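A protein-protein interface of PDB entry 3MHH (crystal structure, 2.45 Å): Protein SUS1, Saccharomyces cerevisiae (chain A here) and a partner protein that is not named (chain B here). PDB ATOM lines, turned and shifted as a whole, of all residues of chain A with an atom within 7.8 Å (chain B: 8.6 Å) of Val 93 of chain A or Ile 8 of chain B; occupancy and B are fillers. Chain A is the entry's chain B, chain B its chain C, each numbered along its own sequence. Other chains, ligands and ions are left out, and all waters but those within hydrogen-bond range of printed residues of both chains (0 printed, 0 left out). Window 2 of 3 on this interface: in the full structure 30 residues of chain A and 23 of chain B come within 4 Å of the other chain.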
ATOM      1  N   LEU A   8      -4.880  -5.180   6.210  1.00  0.00           N
ATOM      2  CA  LEU A   8      -3.944  -5.282   5.111  1.00  0.00           C
ATOM      3  C   LEU A   8      -4.118  -6.611   4.391  1.00  0.00           C
ATOM      4  O   LEU A   8      -4.114  -6.676   3.155  1.00  0.00           O
ATOM      5  CB  LEU A   8      -2.521  -5.171   5.655  1.00  0.00           C
ATOM      6  CG  LEU A   8      -1.374  -5.125   4.652  1.00  0.00           C
ATOM      7  CD1 LEU A   8      -1.562  -3.970   3.677  1.00  0.00           C
ATOM      8  CD2 LEU A   8      -0.059  -4.986   5.409  1.00  0.00           C
ATOM      9  N   ILE A  12      -5.575  -7.239   0.506  1.00  0.00           N
ATOM     10  CA  ILE A  12      -4.739  -7.873  -0.497  1.00  0.00           C
ATOM     11  C   ILE A  12      -5.442  -9.074  -1.121  1.00  0.00           C
ATOM     12  O   ILE A  12      -5.386  -9.281  -2.344  1.00  0.00           O
ATOM     13  CB  ILE A  12      -3.404  -8.325   0.117  1.00  0.00           C
ATOM     14  CG1 ILE A  12      -2.524  -7.103   0.383  1.00  0.00           C
ATOM     15  CG2 ILE A  12      -2.685  -9.304  -0.811  1.00  0.00           C
ATOM     16  CD1 ILE A  12      -1.194  -7.438   1.002  1.00  0.00           C
ATOM     17  N   TYR A  15      -7.886  -8.004  -3.596  1.00  0.00           N
ATOM     18  CA  TYR A  15      -7.256  -7.692  -4.870  1.00  0.00           C
ATOM     19  C   TYR A  15      -6.961  -8.974  -5.641  1.00  0.00           C
ATOM     20  O   TYR A  15      -7.210  -9.058  -6.843  1.00  0.00           O
ATOM     21  CB  TYR A  15      -5.954  -6.910  -4.676  1.00  0.00           C
ATOM     22  CG  TYR A  15      -5.001  -7.092  -5.827  1.00  0.00           C
ATOM     23  CD1 TYR A  15      -5.184  -6.398  -7.017  1.00  0.00           C
ATOM     24  CD2 TYR A  15      -3.951  -7.996  -5.749  1.00  0.00           C
ATOM     25  CE1 TYR A  15      -4.346  -6.582  -8.084  1.00  0.00           C
ATOM     26  CE2 TYR A  15      -3.088  -8.181  -6.815  1.00  0.00           C
ATOM     27  CZ  TYR A  15      -3.296  -7.474  -7.979  1.00  0.00           C
ATOM     28  OH  TYR A  15      -2.455  -7.659  -9.044  1.00  0.00           O
ATOM     29  N   LEU A  82       4.630 -20.112  -2.538  1.00  0.00           N
ATOM     30  CA  LEU A  82       5.063 -18.913  -1.825  1.00  0.00           C
ATOM     31  C   LEU A  82       5.680 -17.910  -2.792  1.00  0.00           C
ATOM     32  O   LEU A  82       5.306 -16.743  -2.807  1.00  0.00           O
ATOM     33  CB  LEU A  82       6.079 -19.247  -0.729  1.00  0.00           C
ATOM     34  CG  LEU A  82       5.508 -19.465   0.670  1.00  0.00           C
ATOM     35  CD1 LEU A  82       6.656 -19.546   1.677  1.00  0.00           C
ATOM     36  CD2 LEU A  82       4.526 -18.357   1.035  1.00  0.00           C
ATOM     37  N   LYS A  83       6.634 -18.368  -3.592  1.00  0.00           N
ATOM     38  CA  LYS A  83       7.292 -17.499  -4.558  1.00  0.00           C
ATOM     39  C   LYS A  83       6.250 -16.806  -5.448  1.00  0.00           C
ATOM     40  O   LYS A  83       6.334 -15.611  -5.691  1.00  0.00           O
ATOM     41  CB  LYS A  83       8.276 -18.312  -5.405  1.00  0.00           C
ATOM     42  CG  LYS A  83       8.935 -17.539  -6.553  1.00  0.00           C
ATOM     43  CD  LYS A  83      10.131 -18.299  -7.130  1.00  0.00           C
ATOM     44  CE  LYS A  83      11.116 -17.357  -7.824  1.00  0.00           C
ATOM     45  NZ  LYS A  83      12.523 -17.870  -7.822  1.00  0.00           N
ATOM     46  N   ILE A  85       2.953 -16.316  -4.843  1.00  0.00           N
ATOM     47  CA  ILE A  85       2.163 -15.373  -4.078  1.00  0.00           C
ATOM     48  C   ILE A  85       2.973 -14.093  -3.878  1.00  0.00           C
ATOM     49  O   ILE A  85       2.438 -12.991  -3.975  1.00  0.00           O
ATOM     50  CB  ILE A  85       1.739 -15.949  -2.708  1.00  0.00           C
ATOM     51  CG1 ILE A  85       0.740 -17.110  -2.896  1.00  0.00           C
ATOM     52  CG2 ILE A  85       1.102 -14.867  -1.845  1.00  0.00           C
ATOM     53  CD1 ILE A  85       0.501 -17.917  -1.607  1.00  0.00           C
ATOM     54  N   ARG A  86       4.272 -14.249  -3.631  1.00  0.00           N
ATOM     55  CA  ARG A  86       5.157 -13.120  -3.368  1.00  0.00           C
ATOM     56  C   ARG A  86       5.245 -12.203  -4.581  1.00  0.00           C
ATOM     57  O   ARG A  86       5.222 -10.978  -4.450  1.00  0.00           O
ATOM     58  CB  ARG A  86       6.565 -13.606  -2.991  1.00  0.00           C
ATOM     59  CG  ARG A  86       6.784 -13.842  -1.500  1.00  0.00           C
ATOM     60  CD  ARG A  86       8.243 -14.187  -1.159  1.00  0.00           C
ATOM     61  NE  ARG A  86       8.477 -15.630  -1.097  1.00  0.00           N
ATOM     62  CZ  ARG A  86       9.330 -16.286  -1.878  1.00  0.00           C
ATOM     63  NH1 ARG A  86      10.056 -15.626  -2.767  1.00  0.00           N
ATOM     64  NH2 ARG A  86       9.469 -17.599  -1.763  1.00  0.00           N
ATOM     65  N   GLU A  87       5.360 -12.801  -5.764  1.00  0.00           N
ATOM     66  CA  GLU A  87       5.521 -12.027  -6.976  1.00  0.00           C
ATOM     67  C   GLU A  87       4.259 -11.211  -7.220  1.00  0.00           C
ATOM     68  O   GLU A  87       4.321 -10.041  -7.571  1.00  0.00           O
ATOM     69  CB  GLU A  87       5.835 -12.937  -8.159  1.00  0.00           C
ATOM     70  CG  GLU A  87       7.278 -13.473  -8.196  1.00  0.00           C
ATOM     71  CD  GLU A  87       7.483 -14.579  -9.239  1.00  0.00           C
ATOM     72  OE1 GLU A  87       8.616 -14.726  -9.713  1.00  0.00           O
ATOM     73  OE2 GLU A  87       6.520 -15.317  -9.580  1.00  0.00           O
ATOM     74  N   PHE A  88       3.102 -11.811  -6.986  1.00  0.00           N
ATOM     75  CA  PHE A  88       1.859 -11.079  -7.149  1.00  0.00           C
ATOM     76  C   PHE A  88       1.807  -9.867  -6.226  1.00  0.00           C
ATOM     77  O   PHE A  88       1.431  -8.782  -6.660  1.00  0.00           O
ATOM     78  CB  PHE A  88       0.663 -11.995  -6.940  1.00  0.00           C
ATOM     79  CG  PHE A  88       0.337 -12.854  -8.138  1.00  0.00           C
ATOM     80  CD1 PHE A  88       0.114 -12.277  -9.381  1.00  0.00           C
ATOM     81  CD2 PHE A  88       0.209 -14.231  -8.010  1.00  0.00           C
ATOM     82  CE1 PHE A  88      -0.208 -13.063 -10.483  1.00  0.00           C
ATOM     83  CE2 PHE A  88      -0.121 -15.028  -9.101  1.00  0.00           C
ATOM     84  CZ  PHE A  88      -0.327 -14.445 -10.341  1.00  0.00           C
ATOM     85  N   LEU A  89       2.242 -10.027  -4.978  1.00  0.00           N
ATOM     86  CA  LEU A  89       2.247  -8.916  -4.013  1.00  0.00           C
ATOM     87  C   LEU A  89       3.326  -7.880  -4.321  1.00  0.00           C
ATOM     88  O   LEU A  89       3.139  -6.696  -4.074  1.00  0.00           O
ATOM     89  CB  LEU A  89       2.444  -9.433  -2.584  1.00  0.00           C
ATOM     90  CG  LEU A  89       1.307 -10.274  -1.999  1.00  0.00           C
ATOM     91  CD1 LEU A  89       1.654 -10.766  -0.612  1.00  0.00           C
ATOM     92  CD2 LEU A  89       0.040  -9.454  -1.959  1.00  0.00           C
ATOM     93  N   GLU A  90       4.463  -8.328  -4.840  1.00  0.00           N
ATOM     94  CA  GLU A  90       5.533  -7.407  -5.227  1.00  0.00           C
ATOM     95  C   GLU A  90       4.968  -6.290  -6.102  1.00  0.00           C
ATOM     96  O   GLU A  90       5.461  -5.173  -6.110  1.00  0.00           O
ATOM     97  CB  GLU A  90       6.624  -8.158  -5.997  1.00  0.00           C
ATOM     98  CG  GLU A  90       7.728  -8.769  -5.121  1.00  0.00           C
ATOM     99  CD  GLU A  90       8.604  -9.774  -5.870  1.00  0.00           C
ATOM    100  OE1 GLU A  90       9.171 -10.668  -5.209  1.00  0.00           O
ATOM    101  OE2 GLU A  90       8.717  -9.678  -7.113  1.00  0.00           O
ATOM    102  N   GLU A  91       3.904  -6.617  -6.813  1.00  0.00           N
ATOM    103  CA  GLU A  91       3.313  -5.764  -7.820  1.00  0.00           C
ATOM    104  C   GLU A  91       2.443  -4.668  -7.206  1.00  0.00           C
ATOM    105  O   GLU A  91       2.237  -3.626  -7.826  1.00  0.00           O
ATOM    106  CB  GLU A  91       2.442  -6.657  -8.722  1.00  0.00           C
ATOM    107  CG  GLU A  91       2.495  -6.370 -10.204  1.00  0.00           C
ATOM    108  CD  GLU A  91       2.132  -7.590 -11.042  1.00  0.00           C
ATOM    109  OE1 GLU A  91       1.055  -8.183 -10.822  1.00  0.00           O
ATOM    110  OE2 GLU A  91       2.930  -7.958 -11.923  1.00  0.00           O
ATOM    111  N   ILE A  92       1.915  -4.907  -6.005  1.00  0.00           N
ATOM    112  CA  ILE A  92       0.913  -4.011  -5.421  1.00  0.00           C
ATOM    113  C   ILE A  92       1.216  -3.492  -4.016  1.00  0.00           C
ATOM    114  O   ILE A  92       0.419  -2.736  -3.462  1.00  0.00           O
ATOM    115  CB  ILE A  92      -0.481  -4.684  -5.359  1.00  0.00           C
ATOM    116  CG1 ILE A  92      -0.507  -5.740  -4.248  1.00  0.00           C
ATOM    117  CG2 ILE A  92      -0.861  -5.285  -6.726  1.00  0.00           C
ATOM    118  CD1 ILE A  92      -1.873  -6.265  -3.948  1.00  0.00           C
ATOM    119  N   VAL A  93       2.330  -3.892  -3.408  1.00  0.00           N
ATOM    120  CA  VAL A  93       2.686  -3.314  -2.109  1.00  0.00           C
ATOM    121  C   VAL A  93       3.903  -2.419  -2.238  1.00  0.00           C
ATOM    122  O   VAL A  93       4.714  -2.588  -3.145  1.00  0.00           O
ATOM    123  CB  VAL A  93       2.950  -4.386  -1.019  1.00  0.00           C
ATOM    124  CG1 VAL A  93       1.890  -5.460  -1.062  1.00  0.00           C
ATOM    125  CG2 VAL A  93       4.350  -4.978  -1.156  1.00  0.00           C
ATOM    126  N   ASP A  94       4.011  -1.445  -1.342  1.00  0.00           N
ATOM    127  CA  ASP A  94       5.212  -0.627  -1.254  1.00  0.00           C
ATOM    128  C   ASP A  94       5.963  -1.040  -0.007  1.00  0.00           C
ATOM    129  O   ASP A  94       5.358  -1.485   0.969  1.00  0.00           O
ATOM    130  CB  ASP A  94       4.859   0.854  -1.181  1.00  0.00           C
ATOM    131  CG  ASP A  94       4.215   1.356  -2.446  1.00  0.00           C
ATOM    132  OD1 ASP A  94       4.669   0.948  -3.536  1.00  0.00           O
ATOM    133  OD2 ASP A  94       3.256   2.154  -2.356  1.00  0.00           O
ATOM    134  N   THR A  95       7.283  -0.897  -0.042  1.00  0.00           N
ATOM    135  CA  THR A  95       8.121  -1.324   1.068  1.00  0.00           C
ATOM    136  C   THR A  95       9.042  -0.193   1.512  1.00  0.00           C
ATOM    137  O   THR A  95       9.269   0.760   0.768  1.00  0.00           O
ATOM    138  CB  THR A  95       8.952  -2.574   0.688  1.00  0.00           C
ATOM    139  OG1 THR A  95       9.788  -2.278  -0.436  1.00  0.00           O
ATOM    140  CG2 THR A  95       8.046  -3.731   0.340  1.00  0.00           C
ATOM    141  N   THR B   5       6.917  -7.562  12.696  1.00  0.00           N
ATOM    142  CA  THR B   5       6.984  -6.585  11.614  1.00  0.00           C
ATOM    143  C   THR B   5       6.517  -7.221  10.302  1.00  0.00           C
ATOM    144  O   THR B   5       7.257  -7.961   9.656  1.00  0.00           O
ATOM    145  CB  THR B   5       8.412  -6.029  11.452  1.00  0.00           C
ATOM    146  OG1 THR B   5       8.929  -5.654  12.736  1.00  0.00           O
ATOM    147  CG2 THR B   5       8.412  -4.815  10.532  1.00  0.00           C
ATOM    148  N   ILE B   6       5.284  -6.919   9.912  1.00  0.00           N
ATOM    149  CA  ILE B   6       4.650  -7.590   8.785  1.00  0.00           C
ATOM    150  C   ILE B   6       5.320  -7.277   7.439  1.00  0.00           C
ATOM    151  O   ILE B   6       5.558  -6.113   7.095  1.00  0.00           O
ATOM    152  CB  ILE B   6       3.143  -7.287   8.750  1.00  0.00           C
ATOM    153  CG1 ILE B   6       2.887  -5.808   8.474  1.00  0.00           C
ATOM    154  CG2 ILE B   6       2.507  -7.665  10.087  1.00  0.00           C
ATOM    155  CD1 ILE B   6       1.473  -5.379   8.850  1.00  0.00           C
ATOM    156  N   THR B   7       5.651  -8.336   6.703  1.00  0.00           N
ATOM    157  CA  THR B   7       6.364  -8.212   5.435  1.00  0.00           C
ATOM    158  C   THR B   7       5.643  -8.977   4.333  1.00  0.00           C
ATOM    159  O   THR B   7       4.678  -9.708   4.592  1.00  0.00           O
ATOM    160  CB  THR B   7       7.784  -8.799   5.533  1.00  0.00           C
ATOM    161  OG1 THR B   7       7.705 -10.221   5.684  1.00  0.00           O
ATOM    162  CG2 THR B   7       8.558  -8.190   6.710  1.00  0.00           C
ATOM    163  N   ILE B   8       6.135  -8.831   3.106  1.00  0.00           N
ATOM    164  CA  ILE B   8       5.558  -9.548   1.978  1.00  0.00           C
ATOM    165  C   ILE B   8       5.633 -11.034   2.236  1.00  0.00           C
ATOM    166  O   ILE B   8       4.743 -11.775   1.838  1.00  0.00           O
ATOM    167  CB  ILE B   8       6.259  -9.247   0.642  1.00  0.00           C
ATOM    168  CG1 ILE B   8       5.937  -7.835   0.174  1.00  0.00           C
ATOM    169  CG2 ILE B   8       5.776 -10.214  -0.440  1.00  0.00           C
ATOM    170  CD1 ILE B   8       6.487  -7.513  -1.214  1.00  0.00           C
ATOM    171  N   ASP B   9       6.700 -11.467   2.909  1.00  0.00           N
ATOM    172  CA  ASP B   9       6.856 -12.883   3.257  1.00  0.00           C
ATOM    173  C   ASP B   9       5.827 -13.350   4.272  1.00  0.00           C
ATOM    174  O   ASP B   9       5.273 -14.430   4.132  1.00  0.00           O
ATOM    175  CB  ASP B   9       8.262 -13.183   3.775  1.00  0.00           C
ATOM    176  CG  ASP B   9       9.254 -13.439   2.654  1.00  0.00           C
ATOM    177  OD1 ASP B   9      10.461 -13.172   2.847  1.00  0.00           O
ATOM    178  OD2 ASP B   9       8.827 -13.902   1.576  1.00  0.00           O
ATOM    179  N   SER B  10       5.570 -12.537   5.288  1.00  0.00           N
ATOM    180  CA  SER B  10       4.638 -12.923   6.337  1.00  0.00           C
ATOM    181  C   SER B  10       3.213 -12.885   5.808  1.00  0.00           C
ATOM    182  O   SER B  10       2.407 -13.760   6.113  1.00  0.00           O
ATOM    183  CB  SER B  10       4.786 -12.020   7.574  1.00  0.00           C
ATOM    184  OG  SER B  10       4.090 -10.793   7.435  1.00  0.00           O
ATOM    185  N   ILE B  11       2.892 -11.880   5.007  1.00  0.00           N
ATOM    186  CA  ILE B  11       1.571 -11.828   4.411  1.00  0.00           C
ATOM    187  C   ILE B  11       1.386 -13.055   3.528  1.00  0.00           C
ATOM    188  O   ILE B  11       0.344 -13.712   3.586  1.00  0.00           O
ATOM    189  CB  ILE B  11       1.342 -10.556   3.570  1.00  0.00           C
ATOM    190  CG1 ILE B  11       1.254  -9.332   4.480  1.00  0.00           C
ATOM    191  CG2 ILE B  11       0.060 -10.675   2.774  1.00  0.00           C
ATOM    192  CD1 ILE B  11       0.173  -9.454   5.546  1.00  0.00           C
ATOM    193  N   SER B  12       2.411 -13.363   2.736  1.00  0.00           N
ATOM    194  CA  SER B  12       2.375 -14.495   1.825  1.00  0.00           C
ATOM    195  C   SER B  12       2.222 -15.827   2.537  1.00  0.00           C
ATOM    196  O   SER B  12       1.398 -16.648   2.140  1.00  0.00           O
ATOM    197  CB  SER B  12       3.611 -14.514   0.932  1.00  0.00           C
ATOM    198  OG  SER B  12       3.475 -13.568  -0.115  1.00  0.00           O
ATOM    199  N   ASN B  13       2.992 -16.052   3.593  1.00  0.00           N
ATOM    200  CA  ASN B  13       2.801 -17.265   4.377  1.00  0.00           C
ATOM    201  C   ASN B  13       1.365 -17.302   4.896  1.00  0.00           C
ATOM    202  O   ASN B  13       0.703 -18.339   4.856  1.00  0.00           O
ATOM    203  CB  ASN B  13       3.807 -17.352   5.524  1.00  0.00           C
ATOM    204  CG  ASN B  13       5.196 -17.772   5.054  1.00  0.00           C
ATOM    205  OD1 ASN B  13       5.413 -18.924   4.670  1.00  0.00           O
ATOM    206  ND2 ASN B  13       6.148 -16.842   5.097  1.00  0.00           N
ATOM    207  N   GLY B  14       0.867 -16.150   5.329  1.00  0.00           N
ATOM    208  CA  GLY B  14      -0.505 -16.055   5.820  1.00  0.00           C
ATOM    209  C   GLY B  14      -1.520 -16.440   4.760  1.00  0.00           C
ATOM    210  O   GLY B  14      -2.501 -17.129   5.049  1.00  0.00           O
ATOM    211  N   ILE B  15      -1.292 -15.984   3.531  1.00  0.00           N
ATOM    212  CA  ILE B  15      -2.176 -16.330   2.416  1.00  0.00           C
ATOM    213  C   ILE B  15      -2.092 -17.826   2.119  1.00  0.00           C
ATOM    214  O   ILE B  15      -3.110 -18.479   1.969  1.00  0.00           O
ATOM    215  CB  ILE B  15      -1.844 -15.511   1.162  1.00  0.00           C
ATOM    216  CG1 ILE B  15      -2.187 -14.044   1.402  1.00  0.00           C
ATOM    217  CG2 ILE B  15      -2.590 -16.032  -0.069  1.00  0.00           C
ATOM    218  CD1 ILE B  15      -1.718 -13.141   0.292  1.00  0.00           C
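The guanidinium group of Arg 86 of chain A is in salt-bridge range of the side-chain carboxylate of Asp 9 of chain B (3.2 Å).
OG1 of Thr 7 of chain B lies close to N of Asp 9 of chain B, at 3.2 Å.
The side-chain hydroxyl of Ser 12 of chain B sits at hydrogen-bond distance from the backbone carbonyl oxygen of Ile 8 of chain B (2.9 Å).
The side-chain amide nitrogen (ND2) of Asn 13 of chain B sits at hydrogen-bond distance from the backbone carbonyl oxygen (O) of Asp 9 of chain B (2.7 Å).
Among the printed residues, merely in contact across the chains: Ile 85 of chain A with Ser 12 of chain B, Leu 82 of chain A with Asn 13 of chain B, Val 93 of chain A with Ile 8 of chain B, Leu 89 of chain A with Ser 12 of chain B, Arg 86 of chain A with Ser 12 of chain B, Leu 82 of chain A with Ser 12 of chain B, Leu 89 of chain A with Ile 11 of chain B, Leu 8 of chain A with Ile 6 of chain B, Ile 12 of chain A with Ile 11 of chain B, Arg 86 of chain A with Ile 8 of chain B and Ile 85 of chain A with Ile 15 of chain B.
Of the printed residues of chain B, Ile 12 of chain A touches Ile 11 (3.9 Å).
Tyr 15 of chain A touches none of the printed residues of chain B.
Lys 83 of chain A touches none of the printed residues of chain B.
Of chain B, only Ile 8 (3.3 Å) comes within 4 Å of Val 93 of chain A.
Of the printed residues of chain A, Ile 6 of chain B touches Leu 8.
Of the printed residues of chain A, Ser 12 of chain B touches Leu 82, Ile 85, Arg 86 and Leu 89.
Of the printed residues of chain A, Asn 13 of chain B touches Leu 82 (3.3 Å).
The nearest printed residue of chain A that does not touch Ile 8 of chain B is Leu 89 of chain A (4.04 Å).
The nearest printed residue of chain B that does not touch Ile 12 of chain A is Ile 15 of chain B (4.1 Å).
Hydrophobic or aromatic side chains of chain B that line the printed part of chain A: Ile 6, Ile 8, Ile 11 and Ile 15.
Along chain B the printed residues that touch a printed residue of chain A span positions 6 to 15.
Printed residues of chain A that touch a printed residue of chain B: Leu 8, Ile 12, Leu 82, Ile 85, Arg 86, Leu 89 and Val 93.
Among the printed residues, 12 pairs touch across the chains.
Among the printed residues, Asp or Glu carboxylates within 4 Å of a Lys or Arg side-chain nitrogen of the other chain: Arg 86 of chain A with Asp 9 of chain B.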
